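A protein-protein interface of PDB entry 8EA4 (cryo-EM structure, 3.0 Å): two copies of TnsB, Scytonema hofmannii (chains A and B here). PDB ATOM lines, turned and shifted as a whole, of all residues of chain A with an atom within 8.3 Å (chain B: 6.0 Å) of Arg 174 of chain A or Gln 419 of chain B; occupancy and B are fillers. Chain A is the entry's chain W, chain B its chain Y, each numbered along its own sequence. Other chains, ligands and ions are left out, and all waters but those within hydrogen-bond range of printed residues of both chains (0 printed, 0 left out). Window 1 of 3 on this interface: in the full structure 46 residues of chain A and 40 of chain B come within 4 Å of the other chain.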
ATOM      1  N   LYS A 169      20.948  -1.763 -20.262  1.00  0.00           N
ATOM      2  CA  LYS A 169      19.622  -1.176 -20.181  1.00  0.00           C
ATOM      3  C   LYS A 169      19.200  -1.021 -18.725  1.00  0.00           C
ATOM      4  O   LYS A 169      18.754   0.063 -18.366  1.00  0.00           O
ATOM      5  CB  LYS A 169      18.640  -2.022 -21.002  1.00  0.00           C
ATOM      6  CG  LYS A 169      18.996  -1.975 -22.497  1.00  0.00           C
ATOM      7  CD  LYS A 169      17.887  -2.593 -23.354  1.00  0.00           C
ATOM      8  CE  LYS A 169      18.065  -2.309 -24.852  1.00  0.00           C
ATOM      9  NZ  LYS A 169      19.044  -3.206 -25.514  1.00  0.00           N
ATOM     10  N   ALA A 170      19.465  -2.005 -17.861  1.00  0.00           N
ATOM     11  CA  ALA A 170      19.037  -1.998 -16.445  1.00  0.00           C
ATOM     12  C   ALA A 170      19.656  -0.803 -15.715  1.00  0.00           C
ATOM     13  O   ALA A 170      19.015  -0.282 -14.790  1.00  0.00           O
ATOM     14  CB  ALA A 170      19.433  -3.293 -15.792  1.00  0.00           C
ATOM     15  N   LYS A 171      20.870  -0.410 -16.101  1.00  0.00           N
ATOM     16  CA  LYS A 171      21.577   0.695 -15.399  1.00  0.00           C
ATOM     17  C   LYS A 171      20.975   2.030 -15.848  1.00  0.00           C
ATOM     18  O   LYS A 171      21.224   3.042 -15.173  1.00  0.00           O
ATOM     19  CB  LYS A 171      23.078   0.666 -15.684  1.00  0.00           C
ATOM     20  CG  LYS A 171      23.466   1.143 -17.077  1.00  0.00           C
ATOM     21  CD  LYS A 171      24.953   0.951 -17.333  1.00  0.00           C
ATOM     22  CE  LYS A 171      25.380   1.601 -18.640  1.00  0.00           C
ATOM     23  NZ  LYS A 171      26.784   1.268 -18.998  1.00  0.00           N
ATOM     24  N   SER A 172      20.250   2.090 -16.966  1.00  0.00           N
ATOM     25  CA  SER A 172      19.862   3.337 -17.646  1.00  0.00           C
ATOM     26  C   SER A 172      18.394   3.737 -17.477  1.00  0.00           C
ATOM     27  O   SER A 172      17.977   4.753 -18.024  1.00  0.00           O
ATOM     28  CB  SER A 172      20.186   3.213 -19.135  1.00  0.00           C
ATOM     29  OG  SER A 172      19.230   2.406 -19.796  1.00  0.00           O
ATOM     30  N   ILE A 173      17.592   2.936 -16.770  1.00  0.00           N
ATOM     31  CA  ILE A 173      16.133   3.081 -16.693  1.00  0.00           C
ATOM     32  C   ILE A 173      15.738   4.475 -16.200  1.00  0.00           C
ATOM     33  O   ILE A 173      16.198   4.915 -15.148  1.00  0.00           O
ATOM     34  CB  ILE A 173      15.538   2.004 -15.767  1.00  0.00           C
ATOM     35  CG1 ILE A 173      15.905   0.563 -16.157  1.00  0.00           C
ATOM     36  CG2 ILE A 173      14.018   2.142 -15.696  1.00  0.00           C
ATOM     37  CD1 ILE A 173      15.414   0.119 -17.527  1.00  0.00           C
ATOM     38  N   ARG A 174      14.867   5.158 -16.940  1.00  0.00           N
ATOM     39  CA  ARG A 174      14.317   6.467 -16.576  1.00  0.00           C
ATOM     40  C   ARG A 174      13.075   6.311 -15.696  1.00  0.00           C
ATOM     41  O   ARG A 174      12.273   5.416 -15.959  1.00  0.00           O
ATOM     42  CB  ARG A 174      14.036   7.225 -17.878  1.00  0.00           C
ATOM     43  CG  ARG A 174      13.820   8.709 -17.613  1.00  0.00           C
ATOM     44  CD  ARG A 174      13.618   9.499 -18.897  1.00  0.00           C
ATOM     45  NE  ARG A 174      13.608  10.930 -18.592  1.00  0.00           N
ATOM     46  CZ  ARG A 174      12.627  11.636 -18.074  1.00  0.00           C
ATOM     47  NH1 ARG A 174      11.430  11.184 -17.889  1.00  0.00           N
ATOM     48  NH2 ARG A 174      12.845  12.857 -17.708  1.00  0.00           N
ATOM     49  N   SER A 175      12.861   7.167 -14.698  1.00  0.00           N
ATOM     50  CA  SER A 175      11.594   7.183 -13.921  1.00  0.00           C
ATOM     51  C   SER A 175      10.659   8.271 -14.450  1.00  0.00           C
ATOM     52  O   SER A 175      11.126   9.398 -14.656  1.00  0.00           O
ATOM     53  CB  SER A 175      11.869   7.414 -12.448  1.00  0.00           C
ATOM     54  OG  SER A 175      12.651   6.382 -11.915  1.00  0.00           O
ATOM     55  N   PRO A 176       9.348   8.032 -14.580  1.00  0.00           N
ATOM     56  CA  PRO A 176       8.419   9.036 -15.084  1.00  0.00           C
ATOM     57  C   PRO A 176       8.367  10.327 -14.269  1.00  0.00           C
ATOM     58  O   PRO A 176       8.102  11.389 -14.829  1.00  0.00           O
ATOM     59  CB  PRO A 176       7.048   8.363 -15.063  1.00  0.00           C
ATOM     60  CG  PRO A 176       7.372   6.885 -15.163  1.00  0.00           C
ATOM     61  CD  PRO A 176       8.666   6.770 -14.382  1.00  0.00           C
ATOM     62  N   GLY A 177       8.616  10.263 -12.958  1.00  0.00           N
ATOM     63  CA  GLY A 177       8.530  11.451 -12.088  1.00  0.00           C
ATOM     64  C   GLY A 177       7.078  11.759 -11.784  1.00  0.00           C
ATOM     65  O   GLY A 177       6.238  10.888 -12.058  1.00  0.00           O
ATOM     66  N   ARG A 179       3.485  14.025 -12.253  1.00  0.00           N
ATOM     67  CA  ARG A 179       2.839  14.774 -13.327  1.00  0.00           C
ATOM     68  C   ARG A 179       2.431  16.183 -12.915  1.00  0.00           C
ATOM     69  O   ARG A 179       2.293  17.020 -13.802  1.00  0.00           O
ATOM     70  CB  ARG A 179       1.685  13.960 -13.933  1.00  0.00           C
ATOM     71  CG  ARG A 179       2.090  12.578 -14.486  1.00  0.00           C
ATOM     72  CD  ARG A 179       3.401  12.538 -15.284  1.00  0.00           C
ATOM     73  NE  ARG A 179       3.385  13.434 -16.454  1.00  0.00           N
ATOM     74  CZ  ARG A 179       4.428  13.914 -17.102  1.00  0.00           C
ATOM     75  NH1 ARG A 179       5.647  13.657 -16.748  1.00  0.00           N
ATOM     76  NH2 ARG A 179       4.271  14.669 -18.139  1.00  0.00           N
ATOM     77  N   ARG A 322      18.251  17.364  -6.369  1.00  0.00           N
ATOM     78  CA  ARG A 322      18.456  17.906  -7.709  1.00  0.00           C
ATOM     79  C   ARG A 322      19.011  19.329  -7.733  1.00  0.00           C
ATOM     80  O   ARG A 322      19.882  19.584  -8.563  1.00  0.00           O
ATOM     81  CB  ARG A 322      17.172  17.746  -8.529  1.00  0.00           C
ATOM     82  CG  ARG A 322      17.212  18.430  -9.893  1.00  0.00           C
ATOM     83  CD  ARG A 322      18.316  17.883 -10.787  1.00  0.00           C
ATOM     84  NE  ARG A 322      18.655  18.856 -11.828  1.00  0.00           N
ATOM     85  CZ  ARG A 322      18.506  18.708 -13.116  1.00  0.00           C
ATOM     86  NH1 ARG A 322      17.931  17.667 -13.627  1.00  0.00           N
ATOM     87  NH2 ARG A 322      18.936  19.618 -13.929  1.00  0.00           N
ATOM     88  N   THR B 417      10.198   4.983 -25.962  1.00  0.00           N
ATOM     89  CA  THR B 417      10.840   4.173 -24.930  1.00  0.00           C
ATOM     90  C   THR B 417       9.824   3.875 -23.852  1.00  0.00           C
ATOM     91  O   THR B 417       9.239   4.803 -23.306  1.00  0.00           O
ATOM     92  CB  THR B 417      12.020   4.933 -24.323  1.00  0.00           C
ATOM     93  OG1 THR B 417      12.995   5.112 -25.318  1.00  0.00           O
ATOM     94  CG2 THR B 417      12.697   4.191 -23.179  1.00  0.00           C
ATOM     95  N   VAL B 418       9.617   2.610 -23.506  1.00  0.00           N
ATOM     96  CA  VAL B 418       8.746   2.248 -22.386  1.00  0.00           C
ATOM     97  C   VAL B 418       9.422   2.643 -21.069  1.00  0.00           C
ATOM     98  O   VAL B 418      10.450   2.091 -20.696  1.00  0.00           O
ATOM     99  CB  VAL B 418       8.439   0.754 -22.413  1.00  0.00           C
ATOM    100  CG1 VAL B 418       7.484   0.368 -21.284  1.00  0.00           C
ATOM    101  CG2 VAL B 418       7.794   0.299 -23.721  1.00  0.00           C
ATOM    102  N   GLN B 419       8.865   3.603 -20.352  1.00  0.00           N
ATOM    103  CA  GLN B 419       9.340   4.067 -19.047  1.00  0.00           C
ATOM    104  C   GLN B 419       8.795   3.145 -17.940  1.00  0.00           C
ATOM    105  O   GLN B 419       7.846   2.399 -18.189  1.00  0.00           O
ATOM    106  CB  GLN B 419       8.945   5.543 -18.887  1.00  0.00           C
ATOM    107  CG  GLN B 419       9.329   6.362 -20.133  1.00  0.00           C
ATOM    108  CD  GLN B 419       9.163   7.860 -19.984  1.00  0.00           C
ATOM    109  OE1 GLN B 419       9.374   8.441 -18.938  1.00  0.00           O
ATOM    110  NE2 GLN B 419       8.841   8.561 -21.039  1.00  0.00           N
ATOM    111  N   ARG B 420       9.385   3.122 -16.737  1.00  0.00           N
ATOM    112  CA  ARG B 420       9.097   2.052 -15.760  1.00  0.00           C
ATOM    113  C   ARG B 420       7.624   1.923 -15.396  1.00  0.00           C
ATOM    114  O   ARG B 420       6.901   2.909 -15.333  1.00  0.00           O
ATOM    115  CB  ARG B 420       9.982   2.125 -14.509  1.00  0.00           C
ATOM    116  CG  ARG B 420       9.505   3.022 -13.363  1.00  0.00           C
ATOM    117  CD  ARG B 420      10.360   2.806 -12.110  1.00  0.00           C
ATOM    118  NE  ARG B 420      11.790   3.079 -12.340  1.00  0.00           N
ATOM    119  CZ  ARG B 420      12.776   2.204 -12.407  1.00  0.00           C
ATOM    120  NH1 ARG B 420      12.577   0.922 -12.390  1.00  0.00           N
ATOM    121  NH2 ARG B 420      14.004   2.611 -12.495  1.00  0.00           N
ATOM    122  N   GLY B 421       7.183   0.697 -15.138  1.00  0.00           N
ATOM    123  CA  GLY B 421       5.772   0.384 -14.906  1.00  0.00           C
ATOM    124  C   GLY B 421       4.926   0.305 -16.180  1.00  0.00           C
ATOM    125  O   GLY B 421       3.715   0.116 -16.092  1.00  0.00           O
ATOM    126  N   GLY B 422       5.533   0.418 -17.363  1.00  0.00           N
ATOM    127  CA  GLY B 422       4.834   0.315 -18.639  1.00  0.00           C
ATOM    128  C   GLY B 422       4.183   1.623 -19.067  1.00  0.00           C
ATOM    129  O   GLY B 422       2.995   1.632 -19.377  1.00  0.00           O
ATOM    130  N   CYS B 423       4.946   2.712 -19.110  1.00  0.00           N
ATOM    131  CA  CYS B 423       4.451   4.031 -19.490  1.00  0.00           C
ATOM    132  C   CYS B 423       5.086   4.546 -20.777  1.00  0.00           C
ATOM    133  O   CYS B 423       6.235   4.237 -21.064  1.00  0.00           O
ATOM    134  CB  CYS B 423       4.696   5.010 -18.355  1.00  0.00           C
ATOM    135  SG  CYS B 423       3.708   4.515 -16.935  1.00  0.00           S
ATOM    136  N   LEU B 424       4.366   5.347 -21.550  1.00  0.00           N
ATOM    137  CA  LEU B 424       4.807   5.978 -22.796  1.00  0.00           C
ATOM    138  C   LEU B 424       4.382   7.438 -22.799  1.00  0.00           C
ATOM    139  O   LEU B 424       3.303   7.746 -22.311  1.00  0.00           O
ATOM    140  CB  LEU B 424       4.153   5.272 -23.994  1.00  0.00           C
ATOM    141  CG  LEU B 424       4.518   3.797 -24.170  1.00  0.00           C
ATOM    142  CD1 LEU B 424       3.591   3.157 -25.195  1.00  0.00           C
ATOM    143  CD2 LEU B 424       5.944   3.657 -24.672  1.00  0.00           C
ATOM    144  N   GLN B 425       5.169   8.299 -23.455  1.00  0.00           N
ATOM    145  CA  GLN B 425       4.791   9.735 -23.574  1.00  0.00           C
ATOM    146  C   GLN B 425       4.366  10.052 -25.013  1.00  0.00           C
ATOM    147  O   GLN B 425       5.140   9.724 -25.937  1.00  0.00           O
ATOM    148  CB  GLN B 425       5.950  10.635 -23.143  1.00  0.00           C
ATOM    149  CG  GLN B 425       5.587  12.109 -23.103  1.00  0.00           C
ATOM    150  CD  GLN B 425       6.692  12.952 -22.512  1.00  0.00           C
ATOM    151  OE1 GLN B 425       7.706  12.442 -22.046  1.00  0.00           O
ATOM    152  NE2 GLN B 425       6.499  14.262 -22.535  1.00  0.00           N
ATOM    153  N   MET B 430       0.739  11.240 -20.628  1.00  0.00           N
ATOM    154  CA  MET B 430       1.383  10.000 -20.205  1.00  0.00           C
ATOM    155  C   MET B 430       0.401   8.841 -20.323  1.00  0.00           C
ATOM    156  O   MET B 430      -0.701   8.903 -19.781  1.00  0.00           O
ATOM    157  CB  MET B 430       1.895  10.168 -18.778  1.00  0.00           C
ATOM    158  CG  MET B 430       2.768   9.005 -18.317  1.00  0.00           C
ATOM    159  SD  MET B 430       4.316   8.807 -19.221  1.00  0.00           S
ATOM    160  CE  MET B 430       5.169  10.351 -18.840  1.00  0.00           C
ATOM    161  N   ALA B 440       9.812  -2.361 -20.031  1.00  0.00           N
ATOM    162  CA  ALA B 440      10.518  -1.147 -19.628  1.00  0.00           C
ATOM    163  C   ALA B 440      11.957  -1.108 -20.176  1.00  0.00           C
ATOM    164  O   ALA B 440      12.675  -2.107 -20.138  1.00  0.00           O
ATOM    165  CB  ALA B 440      10.472  -1.014 -18.106  1.00  0.00           C
ATOM    166  N   GLY B 441      12.373   0.034 -20.717  1.00  0.00           N
ATOM    167  CA  GLY B 441      13.652   0.221 -21.405  1.00  0.00           C
ATOM    168  C   GLY B 441      13.689  -0.263 -22.857  1.00  0.00           C
ATOM    169  O   GLY B 441      14.600   0.115 -23.585  1.00  0.00           O
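Arg 420 of chain B touches Ile 173 of chain A (NH2 to CG2, 3.2 Å). Arg 174 of chain A touches Gln 419 of chain B. Arg 420 of chain B touches Arg 174 of chain A (N to O, 3.8 Å). Pro 176 of chain A touches Arg 420 of chain B. Arg 179 of chain A touches Met 430 of chain B.
Hydrophobic or aromatic side chains of chain B that line the printed part of chain A: Met 430. Of the 11 printed residues of chain A, 5 touch a printed residue of chain B. Printed residues of chain A that touch a printed residue of chain B: Ile 173, Arg 174, Ser 175, Pro 176 and Arg 179. Among the printed residues, 6 pairs touch across the chains. Among the printed residues, no Asp or Glu carboxylate lies within 4 Å of a Lys or Arg side-chain nitrogen of the other chain.
No position is printed for both chains.
Printed residues of chain B within 4 Å of Arg 174 of chain A: Gln 419 and Arg 420. Printed residues of chain A within 4 Å of Gln 419 of chain B: Arg 174. Of the printed residues of chain B, Arg 179 of chain A touches Met 430. Printed residues of chain B within 4 Å of Pro 176 of chain A: Arg 420. Printed residues of chain B within 4 Å of Ile 173 of chain A: Arg 420. Of the printed residues of chain A, Arg 420 of chain B touches Ile 173, Arg 174, Ser 175 and Pro 176. Of the printed residues of chain A, Met 430 of chain B touches Arg 179 (3.9 Å). The nearest printed residue of chain A that does not touch Gln 419 of chain B is Pro 176 of chain A (4.01 Å). The nearest printed residue of chain B that does not touch Ile 173 of chain A is Gly 441 of chain B (4.3 Å).
OG of Ser 175 of chain A sits at hydrogen-bond distance from NE of Arg 420 of chain B.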
